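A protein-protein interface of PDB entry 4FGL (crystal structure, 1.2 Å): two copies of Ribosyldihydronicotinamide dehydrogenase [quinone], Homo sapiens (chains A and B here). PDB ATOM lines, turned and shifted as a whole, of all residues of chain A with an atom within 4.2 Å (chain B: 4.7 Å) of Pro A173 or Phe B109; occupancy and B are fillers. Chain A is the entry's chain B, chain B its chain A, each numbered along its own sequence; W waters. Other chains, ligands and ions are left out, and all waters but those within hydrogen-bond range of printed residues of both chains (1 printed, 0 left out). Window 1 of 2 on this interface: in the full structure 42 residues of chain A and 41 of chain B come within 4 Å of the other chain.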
ATOM      1  N   TYR A 135       6.790  19.920  29.540  1.00  0.00           N
ATOM      2  CA  TYR A 135       7.472  21.173  29.225  1.00  0.00           C
ATOM      3  C   TYR A 135       8.958  20.873  29.006  1.00  0.00           C
ATOM      4  O   TYR A 135       9.287  20.061  28.139  1.00  0.00           O
ATOM      5  CB  TYR A 135       7.159  22.303  30.226  1.00  0.00           C
ATOM      6  CG  TYR A 135       5.719  22.750  30.108  1.00  0.00           C
ATOM      7  CD1 TYR A 135       5.231  23.282  28.917  1.00  0.00           C
ATOM      8  CD2 TYR A 135       4.861  22.655  31.169  1.00  0.00           C
ATOM      9  CE1 TYR A 135       3.936  23.684  28.785  1.00  0.00           C
ATOM     10  CE2 TYR A 135       3.539  23.061  31.054  1.00  0.00           C
ATOM     11  CZ  TYR A 135       3.087  23.583  29.850  1.00  0.00           C
ATOM     12  OH  TYR A 135       1.781  23.991  29.721  1.00  0.00           O
ATOM     13  N   PHE A 170      -3.779  33.173  19.593  1.00  0.00           N
ATOM     14  CA  PHE A 170      -4.336  31.863  19.258  1.00  0.00           C
ATOM     15  C   PHE A 170      -3.267  30.773  19.176  1.00  0.00           C
ATOM     16  O   PHE A 170      -3.590  29.583  19.163  1.00  0.00           O
ATOM     17  CB  PHE A 170      -5.228  31.903  17.994  1.00  0.00           C
ATOM     18  CG  PHE A 170      -4.510  32.147  16.693  1.00  0.00           C
ATOM     19  CD1 PHE A 170      -3.703  31.181  16.119  1.00  0.00           C
ATOM     20  CD2 PHE A 170      -4.728  33.316  15.981  1.00  0.00           C
ATOM     21  CE1 PHE A 170      -3.080  31.411  14.910  1.00  0.00           C
ATOM     22  CE2 PHE A 170      -4.108  33.535  14.760  1.00  0.00           C
ATOM     23  CZ  PHE A 170      -3.293  32.569  14.219  1.00  0.00           C
ATOM     24  N   LEU A 171      -1.992  31.149  19.149  1.00  0.00           N
ATOM     25  CA  LEU A 171      -0.937  30.159  19.093  1.00  0.00           C
ATOM     26  C   LEU A 171      -0.750  29.421  20.412  1.00  0.00           C
ATOM     27  O   LEU A 171      -0.176  28.346  20.427  1.00  0.00           O
ATOM     28  CB  LEU A 171       0.375  30.814  18.652  1.00  0.00           C
ATOM     29  CG  LEU A 171       0.389  31.426  17.254  1.00  0.00           C
ATOM     30  CD1 LEU A 171       1.696  32.140  17.062  1.00  0.00           C
ATOM     31  CD2 LEU A 171       0.229  30.368  16.184  1.00  0.00           C
ATOM     32  N   TRP A 172      -1.202  29.986  21.526  1.00  0.00           N
ATOM     33  CA  TRP A 172      -0.888  29.460  22.845  1.00  0.00           C
ATOM     34  C   TRP A 172      -1.221  27.974  23.049  1.00  0.00           C
ATOM     35  O   TRP A 172      -0.361  27.227  23.491  1.00  0.00           O
ATOM     36  CB  TRP A 172      -1.550  30.347  23.901  1.00  0.00           C
ATOM     37  CG  TRP A 172      -1.409  29.939  25.335  1.00  0.00           C
ATOM     38  CD1 TRP A 172      -2.385  29.439  26.150  1.00  0.00           C
ATOM     39  CD2 TRP A 172      -0.244  30.081  26.157  1.00  0.00           C
ATOM     40  NE1 TRP A 172      -1.900  29.243  27.415  1.00  0.00           N
ATOM     41  CE2 TRP A 172      -0.589  29.642  27.453  1.00  0.00           C
ATOM     42  CE3 TRP A 172       1.052  30.546  25.925  1.00  0.00           C
ATOM     43  CZ2 TRP A 172       0.325  29.637  28.500  1.00  0.00           C
ATOM     44  CZ3 TRP A 172       1.942  30.553  26.974  1.00  0.00           C
ATOM     45  CH2 TRP A 172       1.581  30.105  28.236  1.00  0.00           C
ATOM     46  N   PRO A 173      -2.441  27.526  22.715  1.00  0.00           N
ATOM     47  CA  PRO A 173      -2.726  26.100  22.963  1.00  0.00           C
ATOM     48  C   PRO A 173      -1.854  25.161  22.155  1.00  0.00           C
ATOM     49  O   PRO A 173      -1.551  24.057  22.584  1.00  0.00           O
ATOM     50  CB  PRO A 173      -4.187  25.960  22.553  1.00  0.00           C
ATOM     51  CG  PRO A 173      -4.746  27.325  22.694  1.00  0.00           C
ATOM     52  CD  PRO A 173      -3.641  28.268  22.311  1.00  0.00           C
ATOM     53  N   LEU A 174      -1.471  25.619  20.968  1.00  0.00           N
ATOM     54  CA  LEU A 174      -0.689  24.820  20.030  1.00  0.00           C
ATOM     55  C   LEU A 174       0.793  24.852  20.392  1.00  0.00           C
ATOM     56  O   LEU A 174       1.420  23.826  20.607  1.00  0.00           O
ATOM     57  CB  LEU A 174      -0.877  25.319  18.602  1.00  0.00           C
ATOM     58  CG  LEU A 174      -2.327  25.277  18.100  1.00  0.00           C
ATOM     59  CD1 LEU A 174      -2.453  25.958  16.740  1.00  0.00           C
ATOM     60  CD2 LEU A 174      -2.866  23.874  18.018  1.00  0.00           C
ATOM     61  N   GLN A 175       1.371  26.047  20.489  1.00  0.00           N
ATOM     62  CA  GLN A 175       2.793  26.170  20.775  1.00  0.00           C
ATOM     63  C   GLN A 175       3.128  25.779  22.198  1.00  0.00           C
ATOM     64  O   GLN A 175       4.054  25.012  22.444  1.00  0.00           O
ATOM     65  CB  GLN A 175       3.280  27.592  20.470  1.00  0.00           C
ATOM     66  CG  GLN A 175       3.258  27.858  18.967  1.00  0.00           C
ATOM     67  CD  GLN A 175       3.911  29.162  18.499  1.00  0.00           C
ATOM     68  OE1 GLN A 175       4.302  29.273  17.356  1.00  0.00           O
ATOM     69  NE2 GLN A 175       4.013  30.154  19.382  1.00  0.00           N
ATOM     70  N   GLY A 177       0.712  24.728  24.945  1.00  0.00           N
ATOM     71  CA  GLY A 177      -0.027  23.645  25.545  1.00  0.00           C
ATOM     72  C   GLY A 177       0.239  22.287  24.932  1.00  0.00           C
ATOM     73  O   GLY A 177       0.039  21.277  25.585  1.00  0.00           O
ATOM     74  N   THR A 178       0.685  22.282  23.680  1.00  0.00           N
ATOM     75  CA  THR A 178       0.954  21.037  22.962  1.00  0.00           C
ATOM     76  C   THR A 178       2.441  20.849  22.711  1.00  0.00           C
ATOM     77  O   THR A 178       3.058  19.938  23.261  1.00  0.00           O
ATOM     78  CB  THR A 178       0.156  20.959  21.635  1.00  0.00           C
ATOM     79  OG1 THR A 178      -1.234  21.228  21.894  1.00  0.00           O
ATOM     80  CG2 THR A 178       0.258  19.574  20.990  1.00  0.00           C
ATOM     81  N   LEU B 106     -10.545  18.510  28.555  1.00  0.00           N
ATOM     82  CA  LEU B 106      -9.554  19.279  27.830  1.00  0.00           C
ATOM     83  C   LEU B 106      -8.524  18.330  27.224  1.00  0.00           C
ATOM     84  O   LEU B 106      -7.897  17.546  27.934  1.00  0.00           O
ATOM     85  CB  LEU B 106      -8.884  20.256  28.794  1.00  0.00           C
ATOM     86  CG  LEU B 106      -8.086  21.412  28.175  1.00  0.00           C
ATOM     87  CD1 LEU B 106      -9.017  22.390  27.501  1.00  0.00           C
ATOM     88  CD2 LEU B 106      -7.270  22.143  29.234  1.00  0.00           C
ATOM     89  N   TYR B 107      -8.371  18.403  25.913  1.00  0.00           N
ATOM     90  CA  TYR B 107      -7.334  17.690  25.184  1.00  0.00           C
ATOM     91  C   TYR B 107      -6.457  18.743  24.506  1.00  0.00           C
ATOM     92  O   TYR B 107      -6.924  19.493  23.658  1.00  0.00           O
ATOM     93  CB  TYR B 107      -7.914  16.780  24.106  1.00  0.00           C
ATOM     94  CG  TYR B 107      -8.519  15.456  24.505  1.00  0.00           C
ATOM     95  CD1 TYR B 107      -8.830  15.105  25.812  1.00  0.00           C
ATOM     96  CD2 TYR B 107      -8.814  14.555  23.512  1.00  0.00           C
ATOM     97  CE1 TYR B 107      -9.404  13.854  26.095  1.00  0.00           C
ATOM     98  CE2 TYR B 107      -9.361  13.336  23.782  1.00  0.00           C
ATOM     99  CZ  TYR B 107      -9.659  12.991  25.046  1.00  0.00           C
ATOM    100  OH  TYR B 107     -10.191  11.723  25.205  1.00  0.00           O
ATOM    101  N   TRP B 108      -5.192  18.807  24.900  1.00  0.00           N
ATOM    102  CA  TRP B 108      -4.217  19.721  24.282  1.00  0.00           C
ATOM    103  C   TRP B 108      -4.723  21.172  24.307  1.00  0.00           C
ATOM    104  O   TRP B 108      -4.743  21.883  23.319  1.00  0.00           O
ATOM    105  CB  TRP B 108      -3.820  19.254  22.878  1.00  0.00           C
ATOM    106  CG  TRP B 108      -3.071  17.943  22.924  1.00  0.00           C
ATOM    107  CD1 TRP B 108      -3.421  16.765  22.328  1.00  0.00           C
ATOM    108  CD2 TRP B 108      -1.863  17.692  23.630  1.00  0.00           C
ATOM    109  NE1 TRP B 108      -2.497  15.787  22.621  1.00  0.00           N
ATOM    110  CE2 TRP B 108      -1.525  16.340  23.423  1.00  0.00           C
ATOM    111  CE3 TRP B 108      -1.021  18.488  24.407  1.00  0.00           C
ATOM    112  CZ2 TRP B 108      -0.373  15.766  23.965  1.00  0.00           C
ATOM    113  CZ3 TRP B 108       0.124  17.925  24.924  1.00  0.00           C
ATOM    114  CH2 TRP B 108       0.427  16.579  24.718  1.00  0.00           C
ATOM    115  N   PHE B 109      -5.129  21.597  25.499  1.00  0.00           N
ATOM    116  CA  PHE B 109      -5.567  22.967  25.745  1.00  0.00           C
ATOM    117  C   PHE B 109      -6.759  23.348  24.860  1.00  0.00           C
ATOM    118  O   PHE B 109      -6.983  24.517  24.618  1.00  0.00           O
ATOM    119  CB  PHE B 109      -4.443  23.997  25.532  1.00  0.00           C
ATOM    120  CG  PHE B 109      -3.469  24.183  26.712  1.00  0.00           C
ATOM    121  CD1 PHE B 109      -3.103  23.147  27.554  1.00  0.00           C
ATOM    122  CD2 PHE B 109      -2.909  25.439  26.940  1.00  0.00           C
ATOM    123  CE1 PHE B 109      -2.175  23.384  28.594  1.00  0.00           C
ATOM    124  CE2 PHE B 109      -2.004  25.667  27.957  1.00  0.00           C
ATOM    125  CZ  PHE B 109      -1.635  24.652  28.776  1.00  0.00           C
ATOM    126  N   SER B 110      -7.535  22.354  24.442  1.00  0.00           N
ATOM    127  CA  SER B 110      -8.637  22.588  23.526  1.00  0.00           C
ATOM    128  C   SER B 110      -9.662  21.466  23.665  1.00  0.00           C
ATOM    129  O   SER B 110      -9.673  20.702  24.641  1.00  0.00           O
ATOM    130  CB  SER B 110      -8.076  22.689  22.093  1.00  0.00           C
ATOM    131  OG  SER B 110      -9.090  22.967  21.145  1.00  0.00           O
ATOM    132  N   TYR B 158      -2.905  25.964  36.398  1.00  0.00           N
ATOM    133  CA  TYR B 158      -3.605  26.898  35.524  1.00  0.00           C
ATOM    134  C   TYR B 158      -3.749  28.264  36.177  1.00  0.00           C
ATOM    135  O   TYR B 158      -4.829  28.861  36.218  1.00  0.00           O
ATOM    136  CB  TYR B 158      -4.968  26.331  35.134  1.00  0.00           C
ATOM    137  CG  TYR B 158      -4.874  25.234  34.102  1.00  0.00           C
ATOM    138  CD1 TYR B 158      -4.561  25.521  32.780  1.00  0.00           C
ATOM    139  CD2 TYR B 158      -5.108  23.924  34.442  1.00  0.00           C
ATOM    140  CE1 TYR B 158      -4.467  24.513  31.836  1.00  0.00           C
ATOM    141  CE2 TYR B 158      -5.026  22.920  33.506  1.00  0.00           C
ATOM    142  CZ  TYR B 158      -4.710  23.221  32.201  1.00  0.00           C
ATOM    143  OH  TYR B 158      -4.611  22.241  31.231  1.00  0.00           O
ATOM    144  N   ASN B 164       1.064  26.112  33.302  1.00  0.00           N
ATOM    145  CA  ASN B 164       0.152  26.167  32.163  1.00  0.00           C
ATOM    146  C   ASN B 164      -0.347  27.562  31.862  1.00  0.00           C
ATOM    147  O   ASN B 164      -0.977  27.775  30.829  1.00  0.00           O
ATOM    148  CB  ASN B 164      -1.072  25.303  32.388  1.00  0.00           C
ATOM    149  CG  ASN B 164      -0.763  23.841  32.427  1.00  0.00           C
ATOM    150  OD1 ASN B 164       0.220  23.360  31.843  1.00  0.00           O
ATOM    151  ND2 ASN B 164      -1.600  23.100  33.126  1.00  0.00           N
ATOM    152  N   PHE B 170      -6.276  29.674  27.546  1.00  0.00           N
ATOM    153  CA  PHE B 170      -6.627  28.667  26.566  1.00  0.00           C
ATOM    154  C   PHE B 170      -8.071  28.780  26.099  1.00  0.00           C
ATOM    155  O   PHE B 170      -8.439  28.186  25.087  1.00  0.00           O
ATOM    156  CB  PHE B 170      -6.272  27.228  27.026  1.00  0.00           C
ATOM    157  CG  PHE B 170      -7.142  26.661  28.120  1.00  0.00           C
ATOM    158  CD1 PHE B 170      -8.443  26.272  27.873  1.00  0.00           C
ATOM    159  CD2 PHE B 170      -6.615  26.412  29.385  1.00  0.00           C
ATOM    160  CE1 PHE B 170      -9.205  25.729  28.866  1.00  0.00           C
ATOM    161  CE2 PHE B 170      -7.382  25.872  30.389  1.00  0.00           C
ATOM    162  CZ  PHE B 170      -8.687  25.522  30.130  1.00  0.00           C
ATOM    163  N   PRO B 173      -9.466  30.780  21.888  1.00  0.00           N
ATOM    164  CA  PRO B 173      -9.926  30.311  20.572  1.00  0.00           C
ATOM    165  C   PRO B 173     -11.363  29.796  20.580  1.00  0.00           C
ATOM    166  O   PRO B 173     -12.080  29.914  19.583  1.00  0.00           O
ATOM    167  CB  PRO B 173      -8.948  29.167  20.244  1.00  0.00           C
ATOM    168  CG  PRO B 173      -7.727  29.499  21.013  1.00  0.00           C
ATOM    169  CD  PRO B 173      -8.232  30.094  22.310  1.00  0.00           C
HETATM  170  O   HOH W   1      -3.474  28.377  29.733  1.00  0.00           O
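Hydrophobic or aromatic side chains of chain B within 4 Å of the printed part of chain A: Trp B108 and Phe B109.
OD1 of Asn B164 is in hydrogen-bond range of OH of Tyr A135 (2.7 Å).
Among the printed residues, merely in contact across the chains: Tyr A135 with Phe B109 (3.6 Å), Trp A172 with Phe B109 (3.6 Å), Trp A172 with Asn B164 (3.3 Å), Pro A173 with Trp B108 (3.9 Å), Pro A173 with Phe B109 (3.6 Å), Gly A177 with Trp B108 (3.2 Å), Gly A177 with Phe B109 (3.7 Å) and Thr A178 with Trp B108 (3.4 Å).
Of chain B, only Trp B108 (3.9 Å) and Phe B109 (3.6 Å) come within 4 Å of Pro A173.
Phe B109 touches just these residues of chain A: Tyr A135, Trp A172, Pro A173 and Gly A177.
Of the printed residues of chain B, Gly A177 touches Trp B108 and Phe B109.
Printed residues of chain B within 4 Å of Trp A172: Phe B109 (3.6 Å) and Asn B164 (3.3 Å).
Of the printed residues of chain A, Asn B164 touches Tyr A135 and Trp A172.
Tyr B107 touches none of the printed residues of chain A.
Positions printed for both chains: 170 and 173.
Water W1 lies within hydrogen-bond range of O of Asn B164 and NE1 of Trp A172.
The backbone carbonyl oxygen (O) of Pro A173 sits at hydrogen-bond distance from the side-chain hydroxyl (OG1) of Thr A178.
N of Gly A177 sits at hydrogen-bond distance from O of Trp A172, 3.1 Å away.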
